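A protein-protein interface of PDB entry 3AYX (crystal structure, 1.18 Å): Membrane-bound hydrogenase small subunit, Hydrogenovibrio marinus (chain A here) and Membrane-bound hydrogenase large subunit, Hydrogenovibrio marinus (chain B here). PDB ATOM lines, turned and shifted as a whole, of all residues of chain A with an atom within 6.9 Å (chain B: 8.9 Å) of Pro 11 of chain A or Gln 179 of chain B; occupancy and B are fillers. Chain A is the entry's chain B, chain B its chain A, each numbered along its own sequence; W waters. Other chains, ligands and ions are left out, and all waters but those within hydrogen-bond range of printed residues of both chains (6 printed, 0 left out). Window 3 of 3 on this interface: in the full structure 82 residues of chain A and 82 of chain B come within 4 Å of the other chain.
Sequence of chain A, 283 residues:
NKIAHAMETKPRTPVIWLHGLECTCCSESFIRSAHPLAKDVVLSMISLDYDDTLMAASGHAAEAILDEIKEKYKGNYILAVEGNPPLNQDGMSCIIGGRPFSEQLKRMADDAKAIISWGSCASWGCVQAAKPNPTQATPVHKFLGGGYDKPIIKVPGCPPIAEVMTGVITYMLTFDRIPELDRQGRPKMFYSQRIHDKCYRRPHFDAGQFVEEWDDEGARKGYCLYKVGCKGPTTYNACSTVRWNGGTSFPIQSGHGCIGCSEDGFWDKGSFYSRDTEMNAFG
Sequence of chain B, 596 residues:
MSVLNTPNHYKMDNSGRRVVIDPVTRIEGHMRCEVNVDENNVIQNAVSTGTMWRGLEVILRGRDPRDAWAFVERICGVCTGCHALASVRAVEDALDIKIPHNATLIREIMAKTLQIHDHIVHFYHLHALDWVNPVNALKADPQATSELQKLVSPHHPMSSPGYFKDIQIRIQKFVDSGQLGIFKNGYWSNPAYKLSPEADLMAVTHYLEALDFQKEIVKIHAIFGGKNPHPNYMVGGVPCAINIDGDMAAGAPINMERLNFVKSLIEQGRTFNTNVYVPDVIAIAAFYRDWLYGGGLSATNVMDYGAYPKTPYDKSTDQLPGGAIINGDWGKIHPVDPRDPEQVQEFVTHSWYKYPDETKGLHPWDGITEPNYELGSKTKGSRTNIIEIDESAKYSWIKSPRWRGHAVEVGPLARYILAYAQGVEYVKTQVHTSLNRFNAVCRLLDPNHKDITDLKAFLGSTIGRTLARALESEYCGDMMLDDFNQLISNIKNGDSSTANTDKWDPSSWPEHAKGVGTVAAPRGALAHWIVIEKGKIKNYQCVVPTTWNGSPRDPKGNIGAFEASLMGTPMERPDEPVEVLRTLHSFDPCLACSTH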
ATOM      1  N   PRO A  11      17.789   3.031   2.952  1.00  0.00           N
ATOM      2  CA  PRO A  11      16.641   2.089   3.039  1.00  0.00           C
ATOM      3  C   PRO A  11      16.629   1.059   1.953  1.00  0.00           C
ATOM      4  O   PRO A  11      17.006   1.173   0.811  1.00  0.00           O
ATOM      5  CB  PRO A  11      15.356   2.882   2.722  1.00  0.00           C
ATOM      6  CG  PRO A  11      15.965   3.849   1.766  1.00  0.00           C
ATOM      7  CD  PRO A  11      17.218   4.313   2.508  1.00  0.00           C
ATOM      8  N   ARG A  12      16.107  -0.049   2.391  1.00  0.00           N
ATOM      9  CA  ARG A  12      16.252  -1.330   1.721  1.00  0.00           C
ATOM     10  C   ARG A  12      15.069  -1.577   0.843  1.00  0.00           C
ATOM     11  O   ARG A  12      13.939  -1.280   1.269  1.00  0.00           O
ATOM     12  CB  ARG A  12      16.463  -2.509   2.699  1.00  0.00           C
ATOM     13  CG  ARG A  12      17.882  -2.400   3.333  1.00  0.00           C
ATOM     14  CD  ARG A  12      18.057  -3.399   4.487  1.00  0.00           C
ATOM     15  NE  ARG A  12      17.299  -3.056   5.704  1.00  0.00           N
ATOM     16  CZ  ARG A  12      16.260  -3.649   6.260  1.00  0.00           C
ATOM     17  NH1 ARG A  12      15.780  -4.741   5.740  1.00  0.00           N
ATOM     18  NH2 ARG A  12      15.772  -3.137   7.385  1.00  0.00           N
ATOM     19  N   THR A  13      15.301  -2.133  -0.345  1.00  0.00           N
ATOM     20  CA  THR A  13      14.228  -2.298  -1.307  1.00  0.00           C
ATOM     21  C   THR A  13      13.105  -3.158  -0.761  1.00  0.00           C
ATOM     22  O   THR A  13      13.369  -4.322  -0.402  1.00  0.00           O
ATOM     23  CB  THR A  13      14.781  -2.925  -2.603  1.00  0.00           C
ATOM     24  OG1 THR A  13      15.789  -2.072  -3.186  1.00  0.00           O
ATOM     25  CG2 THR A  13      13.718  -3.159  -3.689  1.00  0.00           C
ATOM     26  N   PRO A  14      11.890  -2.699  -0.697  1.00  0.00           N
ATOM     27  CA  PRO A  14      10.793  -3.553  -0.246  1.00  0.00           C
ATOM     28  C   PRO A  14      10.487  -4.651  -1.226  1.00  0.00           C
ATOM     29  O   PRO A  14      10.389  -4.429  -2.420  1.00  0.00           O
ATOM     30  CB  PRO A  14       9.587  -2.609  -0.125  1.00  0.00           C
ATOM     31  CG  PRO A  14      10.251  -1.304  -0.009  1.00  0.00           C
ATOM     32  CD  PRO A  14      11.450  -1.363  -0.909  1.00  0.00           C
ATOM     33  N   VAL A  42      18.244 -10.746   3.795  1.00  0.00           N
ATOM     34  CA  VAL A  42      17.084 -10.306   4.577  1.00  0.00           C
ATOM     35  C   VAL A  42      17.429  -9.203   5.549  1.00  0.00           C
ATOM     36  O   VAL A  42      16.573  -8.261   5.756  1.00  0.00           O
ATOM     37  CB  VAL A  42      16.402 -11.504   5.320  1.00  0.00           C
ATOM     38  CG1 VAL A  42      15.386 -10.942   6.266  1.00  0.00           C
ATOM     39  CG2 VAL A  42      15.855 -12.467   4.249  1.00  0.00           C
ATOM     40  N   LEU A  43      18.608  -9.199   6.136  1.00  0.00           N
ATOM     41  CA  LEU A  43      18.945  -8.164   7.115  1.00  0.00           C
ATOM     42  C   LEU A  43      19.487  -6.892   6.475  1.00  0.00           C
ATOM     43  O   LEU A  43      19.243  -5.802   6.995  1.00  0.00           O
ATOM     44  CB  LEU A  43      19.909  -8.721   8.150  1.00  0.00           C
ATOM     45  CG  LEU A  43      19.379  -9.762   9.096  1.00  0.00           C
ATOM     46  CD1 LEU A  43      20.545 -10.342   9.929  1.00  0.00           C
ATOM     47  CD2 LEU A  43      18.328  -9.187  10.004  1.00  0.00           C
ATOM     48  N   MET A  45      20.098  -6.360   2.574  1.00  0.00           N
ATOM     49  CA  MET A  45      19.973  -6.048   1.157  1.00  0.00           C
ATOM     50  C   MET A  45      18.572  -5.611   0.735  1.00  0.00           C
ATOM     51  O   MET A  45      18.354  -4.586   0.097  1.00  0.00           O
ATOM     52  CB  MET A  45      20.422  -7.202   0.273  1.00  0.00           C
ATOM     53  CG  MET A  45      21.880  -7.545   0.565  1.00  0.00           C
ATOM     54  SD  MET A  45      22.392  -8.822  -0.631  1.00  0.00           S
ATOM     55  CE  MET A  45      24.014  -9.009  -0.011  1.00  0.00           C
ATOM     56  N   ILE A  46      17.570  -6.371   1.059  1.00  0.00           N
ATOM     57  CA  ILE A  46      16.170  -6.106   0.803  1.00  0.00           C
ATOM     58  C   ILE A  46      15.462  -5.899   2.129  1.00  0.00           C
ATOM     59  O   ILE A  46      16.027  -6.121   3.167  1.00  0.00           O
ATOM     60  CB  ILE A  46      15.500  -7.216  -0.025  1.00  0.00           C
ATOM     61  CG1 ILE A  46      15.382  -8.539   0.795  1.00  0.00           C
ATOM     62  CG2 ILE A  46      16.222  -7.350  -1.363  1.00  0.00           C
ATOM     63  CD1 ILE A  46      14.676  -9.696   0.158  1.00  0.00           C
ATOM     64  N   SER A  47      14.206  -5.434   2.033  1.00  0.00           N
ATOM     65  CA  SER A  47      13.305  -5.526   3.165  1.00  0.00           C
ATOM     66  C   SER A  47      12.221  -6.536   2.815  1.00  0.00           C
ATOM     67  O   SER A  47      11.352  -6.211   2.010  1.00  0.00           O
ATOM     68  CB  SER A  47      12.710  -4.131   3.524  1.00  0.00           C
ATOM     69  OG  SER A  47      11.962  -4.203   4.703  1.00  0.00           O
ATOM     70  N   LEU A  48      12.283  -7.722   3.353  1.00  0.00           N
ATOM     71  CA  LEU A  48      11.348  -8.802   3.050  1.00  0.00           C
ATOM     72  C   LEU A  48      10.134  -8.583   3.925  1.00  0.00           C
ATOM     73  O   LEU A  48      10.070  -8.956   5.078  1.00  0.00           O
ATOM     74  CB  LEU A  48      12.025 -10.159   3.296  1.00  0.00           C
ATOM     75  CG  LEU A  48      11.160 -11.389   2.941  1.00  0.00           C
ATOM     76  CD1 LEU A  48      10.733 -11.332   1.486  1.00  0.00           C
ATOM     77  CD2 LEU A  48      11.923 -12.657   3.336  1.00  0.00           C
ATOM     78  N   ASP A  49       9.168  -7.849   3.363  1.00  0.00           N
ATOM     79  CA  ASP A  49       8.114  -7.282   4.167  1.00  0.00           C
ATOM     80  C   ASP A  49       6.903  -8.203   4.305  1.00  0.00           C
ATOM     81  O   ASP A  49       6.126  -7.988   5.226  1.00  0.00           O
ATOM     82  CB  ASP A  49       7.646  -5.978   3.548  1.00  0.00           C
ATOM     83  CG  ASP A  49       8.692  -4.907   3.741  1.00  0.00           C
ATOM     84  OD1 ASP A  49       9.529  -5.008   4.663  1.00  0.00           O
ATOM     85  OD2 ASP A  49       8.710  -3.901   2.977  1.00  0.00           O
ATOM     86  N   LYS A  72       2.229   2.753   1.369  1.00  0.00           N
ATOM     87  CA  LYS A  72       3.459   3.452   1.785  1.00  0.00           C
ATOM     88  C   LYS A  72       4.489   3.372   0.658  1.00  0.00           C
ATOM     89  O   LYS A  72       5.225   4.343   0.398  1.00  0.00           O
ATOM     90  CB  LYS A  72       3.981   2.908   3.112  1.00  0.00           C
ATOM     91  CG  LYS A  72       5.363   3.284   3.647  1.00  0.00           C
ATOM     92  CD  LYS A  72       5.498   3.325   5.184  1.00  0.00           C
ATOM     93  CE  LYS A  72       6.831   3.821   5.725  1.00  0.00           C
ATOM     94  NZ  LYS A  72       7.066   3.614   7.195  1.00  0.00           N
ATOM     95  N   TYR A  73       4.528   2.226  -0.017  1.00  0.00           N
ATOM     96  CA  TYR A  73       5.583   1.971  -1.024  1.00  0.00           C
ATOM     97  C   TYR A  73       4.951   1.747  -2.400  1.00  0.00           C
ATOM     98  O   TYR A  73       5.481   1.069  -3.239  1.00  0.00           O
ATOM     99  CB  TYR A  73       6.407   0.794  -0.546  1.00  0.00           C
ATOM    100  CG  TYR A  73       7.279   1.107   0.666  1.00  0.00           C
ATOM    101  CD1 TYR A  73       8.466   1.783   0.520  1.00  0.00           C
ATOM    102  CD2 TYR A  73       6.957   0.755   1.945  1.00  0.00           C
ATOM    103  CE1 TYR A  73       9.220   2.051   1.659  1.00  0.00           C
ATOM    104  CE2 TYR A  73       7.677   1.005   3.087  1.00  0.00           C
ATOM    105  CZ  TYR A  73       8.850   1.665   2.917  1.00  0.00           C
ATOM    106  OH  TYR A  73       9.611   1.952   4.011  1.00  0.00           O
ATOM    107  N   ILE B 171      20.680  -6.668  15.147  1.00  0.00           N
ATOM    108  CA  ILE B 171      19.225  -6.661  15.249  1.00  0.00           C
ATOM    109  C   ILE B 171      18.745  -5.248  15.629  1.00  0.00           C
ATOM    110  O   ILE B 171      17.728  -4.779  15.116  1.00  0.00           O
ATOM    111  CB  ILE B 171      18.760  -7.748  16.253  1.00  0.00           C
ATOM    112  CG1 ILE B 171      19.203  -9.155  15.923  1.00  0.00           C
ATOM    113  CG2 ILE B 171      17.221  -7.739  16.407  1.00  0.00           C
ATOM    114  CD1 ILE B 171      18.756  -9.596  14.526  1.00  0.00           C
ATOM    115  N   GLN B 172      19.471  -4.575  16.485  1.00  0.00           N
ATOM    116  CA  GLN B 172      19.094  -3.167  16.792  1.00  0.00           C
ATOM    117  C   GLN B 172      19.087  -2.245  15.607  1.00  0.00           C
ATOM    118  O   GLN B 172      18.173  -1.435  15.502  1.00  0.00           O
ATOM    119  CB  GLN B 172      20.024  -2.673  17.926  1.00  0.00           C
ATOM    120  CG  GLN B 172      19.541  -1.312  18.442  1.00  0.00           C
ATOM    121  CD  GLN B 172      18.333  -1.383  19.305  1.00  0.00           C
ATOM    122  OE1 GLN B 172      18.435  -2.003  20.366  1.00  0.00           O
ATOM    123  NE2 GLN B 172      17.222  -0.797  18.927  1.00  0.00           N
ATOM    124  N   LYS B 173      20.105  -2.388  14.729  1.00  0.00           N
ATOM    125  CA  LYS B 173      20.173  -1.591  13.479  1.00  0.00           C
ATOM    126  C   LYS B 173      18.986  -1.892  12.586  1.00  0.00           C
ATOM    127  O   LYS B 173      18.385  -0.970  12.009  1.00  0.00           O
ATOM    128  CB  LYS B 173      21.488  -1.864  12.791  1.00  0.00           C
ATOM    129  CG  LYS B 173      21.897  -1.347  11.451  1.00  0.00           C
ATOM    130  CD  LYS B 173      23.332  -1.797  11.147  1.00  0.00           C
ATOM    131  CE  LYS B 173      23.515  -2.081   9.655  1.00  0.00           C
ATOM    132  NZ  LYS B 173      24.908  -1.816   9.112  1.00  0.00           N
ATOM    133  N   PHE B 174      18.637  -3.168  12.454  1.00  0.00           N
ATOM    134  CA  PHE B 174      17.471  -3.599  11.706  1.00  0.00           C
ATOM    135  C   PHE B 174      16.202  -2.951  12.239  1.00  0.00           C
ATOM    136  O   PHE B 174      15.421  -2.300  11.511  1.00  0.00           O
ATOM    137  CB  PHE B 174      17.426  -5.123  11.748  1.00  0.00           C
ATOM    138  CG  PHE B 174      16.318  -5.763  10.997  1.00  0.00           C
ATOM    139  CD1 PHE B 174      16.467  -6.017   9.627  1.00  0.00           C
ATOM    140  CD2 PHE B 174      15.167  -6.185  11.628  1.00  0.00           C
ATOM    141  CE1 PHE B 174      15.485  -6.671   8.874  1.00  0.00           C
ATOM    142  CE2 PHE B 174      14.151  -6.817  10.872  1.00  0.00           C
ATOM    143  CZ  PHE B 174      14.332  -7.058   9.526  1.00  0.00           C
ATOM    144  N   VAL B 175      15.986  -3.053  13.519  1.00  0.00           N
ATOM    145  CA  VAL B 175      14.795  -2.435  14.124  1.00  0.00           C
ATOM    146  C   VAL B 175      14.853  -0.939  13.989  1.00  0.00           C
ATOM    147  O   VAL B 175      13.831  -0.306  13.670  1.00  0.00           O
ATOM    148  CB  VAL B 175      14.708  -2.916  15.620  1.00  0.00           C
ATOM    149  CG1 VAL B 175      13.669  -2.094  16.390  1.00  0.00           C
ATOM    150  CG2 VAL B 175      14.406  -4.390  15.651  1.00  0.00           C
ATOM    151  N   ASP B 176      16.007  -0.319  14.222  1.00  0.00           N
ATOM    152  CA  ASP B 176      16.097   1.130  14.150  1.00  0.00           C
ATOM    153  C   ASP B 176      15.878   1.669  12.744  1.00  0.00           C
ATOM    154  O   ASP B 176      15.545   2.849  12.492  1.00  0.00           O
ATOM    155  CB  ASP B 176      17.465   1.604  14.599  1.00  0.00           C
ATOM    156  CG  ASP B 176      17.642   1.463  16.084  1.00  0.00           C
ATOM    157  OD1 ASP B 176      16.675   1.215  16.823  1.00  0.00           O
ATOM    158  OD2 ASP B 176      18.791   1.635  16.546  1.00  0.00           O
ATOM    159  N   SER B 177      15.999   0.815  11.766  1.00  0.00           N
ATOM    160  CA  SER B 177      15.744   1.187  10.357  1.00  0.00           C
ATOM    161  C   SER B 177      14.282   1.468  10.103  1.00  0.00           C
ATOM    162  O   SER B 177      13.936   2.113   9.113  1.00  0.00           O
ATOM    163  CB  SER B 177      16.226   0.130   9.376  1.00  0.00           C
ATOM    164  OG  SER B 177      15.319  -0.947   9.255  1.00  0.00           O
ATOM    165  N   GLY B 178      13.422   0.964  10.977  1.00  0.00           N
ATOM    166  CA  GLY B 178      12.005   1.072  10.776  1.00  0.00           C
ATOM    167  C   GLY B 178      11.404   0.125   9.737  1.00  0.00           C
ATOM    168  O   GLY B 178      10.179   0.185   9.539  1.00  0.00           O
ATOM    169  N   GLN B 179      12.229  -0.670   9.084  1.00  0.00           N
ATOM    170  CA  GLN B 179      11.813  -1.711   8.139  1.00  0.00           C
ATOM    171  C   GLN B 179      11.936  -3.055   8.841  1.00  0.00           C
ATOM    172  O   GLN B 179      12.954  -3.673   8.756  1.00  0.00           O
ATOM    173  CB  GLN B 179      12.583  -1.617   6.823  1.00  0.00           C
ATOM    174  CG  GLN B 179      12.336  -0.313   6.106  1.00  0.00           C
ATOM    175  CD  GLN B 179      13.135  -0.312   4.815  1.00  0.00           C
ATOM    176  OE1 GLN B 179      14.310   0.010   4.860  1.00  0.00           O
ATOM    177  NE2 GLN B 179      12.481  -0.721   3.717  1.00  0.00           N
ATOM    178  N   LEU B 180      10.888  -3.452   9.537  1.00  0.00           N
ATOM    179  CA  LEU B 180      11.015  -4.593  10.424  1.00  0.00           C
ATOM    180  C   LEU B 180      10.798  -5.934   9.726  1.00  0.00           C
ATOM    181  O   LEU B 180      11.029  -6.991  10.351  1.00  0.00           O
ATOM    182  CB  LEU B 180      10.035  -4.460  11.612  1.00  0.00           C
ATOM    183  CG  LEU B 180      10.414  -3.518  12.758  1.00  0.00           C
ATOM    184  CD1 LEU B 180      11.010  -4.377  13.889  1.00  0.00           C
ATOM    185  CD2 LEU B 180      11.390  -2.424  12.547  1.00  0.00           C
ATOM    186  N   GLY B 181      10.402  -5.926   8.441  1.00  0.00           N
ATOM    187  CA  GLY B 181      10.372  -7.120   7.651  1.00  0.00           C
ATOM    188  C   GLY B 181       9.631  -8.264   8.278  1.00  0.00           C
ATOM    189  O   GLY B 181       8.493  -8.126   8.632  1.00  0.00           O
ATOM    190  N   ILE B 182      10.317  -9.424   8.417  1.00  0.00           N
ATOM    191  CA  ILE B 182       9.690 -10.647   8.911  1.00  0.00           C
ATOM    192  C   ILE B 182       9.317 -10.508  10.372  1.00  0.00           C
ATOM    193  O   ILE B 182       8.569 -11.326  10.885  1.00  0.00           O
ATOM    194  CB  ILE B 182      10.595 -11.875   8.805  1.00  0.00           C
ATOM    195  CG1 ILE B 182      11.996 -11.711   9.417  1.00  0.00           C
ATOM    196  CG2 ILE B 182      10.734 -12.333   7.374  1.00  0.00           C
ATOM    197  CD1 ILE B 182      12.695 -13.092   9.491  1.00  0.00           C
ATOM    198  N   PHE B 183       9.721  -9.470  11.079  1.00  0.00           N
ATOM    199  CA  PHE B 183       9.291  -9.312  12.467  1.00  0.00           C
ATOM    200  C   PHE B 183       8.132  -8.338  12.649  1.00  0.00           C
ATOM    201  O   PHE B 183       7.547  -8.125  13.711  1.00  0.00           O
ATOM    202  CB  PHE B 183      10.474  -8.850  13.284  1.00  0.00           C
ATOM    203  CG  PHE B 183      11.666  -9.783  13.387  1.00  0.00           C
ATOM    204  CD1 PHE B 183      11.598 -11.133  13.190  1.00  0.00           C
ATOM    205  CD2 PHE B 183      12.936  -9.265  13.699  1.00  0.00           C
ATOM    206  CE1 PHE B 183      12.733 -11.921  13.283  1.00  0.00           C
ATOM    207  CE2 PHE B 183      14.127  -9.994  13.835  1.00  0.00           C
ATOM    208  CZ  PHE B 183      13.974 -11.385  13.607  1.00  0.00           C
ATOM    209  N   LYS B 184       7.759  -7.716  11.547  1.00  0.00           N
ATOM    210  CA  LYS B 184       6.722  -6.694  11.561  1.00  0.00           C
ATOM    211  C   LYS B 184       5.395  -7.286  11.994  1.00  0.00           C
ATOM    212  O   LYS B 184       4.963  -8.329  11.504  1.00  0.00           O
ATOM    213  CB  LYS B 184       6.548  -6.121  10.185  1.00  0.00           C
ATOM    214  CG  LYS B 184       5.745  -4.931   9.784  1.00  0.00           C
ATOM    215  CD  LYS B 184       6.053  -4.830   8.197  1.00  0.00           C
ATOM    216  CE  LYS B 184       6.418  -3.375   7.920  1.00  0.00           C
ATOM    217  NZ  LYS B 184       5.382  -2.474   8.538  1.00  0.00           N
HETATM  218  O   HOH W   1       9.221  -3.829   6.843  1.00  0.00           O
HETATM  219  O   HOH W   2      12.150  -9.588   6.762  1.00  0.00           O
HETATM  220  O   HOH W   3      13.197  -5.512   6.718  1.00  0.00           O
HETATM  221  O   HOH W   4       9.682  -1.632   3.699  1.00  0.00           O
HETATM  222  O   HOH W   5       9.014   1.313   7.079  1.00  0.00           O
HETATM  223  O   HOH W   6       6.698  -9.836   7.438  1.00  0.00           O
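Among the printed residues, no Asp or Glu carboxylate lies within 4 Å of a Lys or Arg side-chain nitrogen of the other chain.
The side-chain hydroxyl (OG) of Ser 177 of chain B lies within hydrogen-bond range of the guanidinium group (NH2) of Arg 12 of chain A, 2.9 Å away.
NE2 of Gln 179 of chain B sits at hydrogen-bond distance from O of Arg 12 of chain A, at 2.9 Å.
N of Ile 182 of chain B sits at hydrogen-bond distance from O of Leu 48 of chain A (3.4 Å).
CA of Pro 11 of chain A touches OE1 of Gln 179 of chain B, 3.6 Å away.
Phe 174 of chain B touches Arg 12 of chain A.
O of Val 42 of chain A touches CE1 of Phe 174 of chain B, 3.7 Å away.
Phe 174 of chain B touches Leu 43 of chain A (CD1 to CD2, 3.7 Å).
Ser 47 of chain A touches Gln 179 of chain B.
Leu 48 of chain A touches Gly 181 of chain B (O to CA, 3.2 Å).
OD1 of Asp 49 of chain A touches CA of Gly 181 of chain B (3.8 Å).
Tyr 73 of chain A touches Gln 179 of chain B (OH to NE2, 3.9 Å).
Water W2 lies within hydrogen-bond range of N of Ile 182 of chain B (2.5 Å) and O of Leu 48 of chain A (2.7 Å).
Water W1 lies within hydrogen-bond range of OD1 of Asp 49 of chain A (2.5 Å), N of Gly 181 of chain B (2.9 Å), N of Leu 180 of chain B (3.2 Å) and OG of Ser 47 of chain A (3.5 Å).
Water W4 lies within hydrogen-bond range of OD2 of Asp 49 of chain A and NE2 of Gln 179 of chain B.
Water W3 lies within hydrogen-bond range of OG of Ser 47 of chain A (2.7 Å), O of Gln 179 of chain B (2.8 Å), NH1 of Arg 12 of chain A (2.9 Å) and N of Gly 181 of chain B (3.3 Å).
Water W6 bridges the backbone carbonyl oxygen (O) of Gly 181 of chain B (2.8 Å) and the backbone carbonyl oxygen (O) of Asp 49 of chain A (2.9 Å).
Water W5 lies within hydrogen-bond range of the backbone carbonyl oxygen of Gly 178 of chain B (2.9 Å), the side-chain amino group of Lys 72 of chain A (3.0 Å) and the side-chain hydroxyl of Tyr 73 of chain A (3.2 Å).
The backbone carbonyl oxygen of Phe 174 of chain B lies within hydrogen-bond range of the side-chain hydroxyl of Ser 177 of chain B, 2.6 Å away.
N of Gln 179 of chain B lies within hydrogen-bond range of OG of Ser 177 of chain B (3.1 Å).
The backbone carbonyl oxygen (O) of Ile 46 of chain A is in hydrogen-bond range of the guanidinium group (NH1) of Arg 12 of chain A (2.9 Å).
O of Thr 13 of chain A sits at hydrogen-bond distance from N of Ser 47 of chain A.
OG of Ser 47 of chain A lies within hydrogen-bond range of OD1 of Asp 49 of chain A, at 2.6 Å.
Of chain B, only Gln 179 (3.6 Å) comes within 4 Å of Pro 11 of chain A.
Printed residues of chain B within 4 Å of Asp 49 of chain A: Gly 181 (3.8 Å).
Of the printed residues of chain A, Phe 174 of chain B touches Arg 12 (3.7 Å), Val 42 (3.7 Å) and Leu 43 (3.7 Å).
Of the printed residues of chain A, Ser 177 of chain B touches Arg 12.
Gln 179 of chain B touches four residues of chain A.
Of the printed residues of chain A, Gly 181 of chain B touches Leu 48 and Asp 49.
The nearest residue of chain A that does not touch Gln 179 of chain B is Pro 14 of chain A (4.4 Å).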
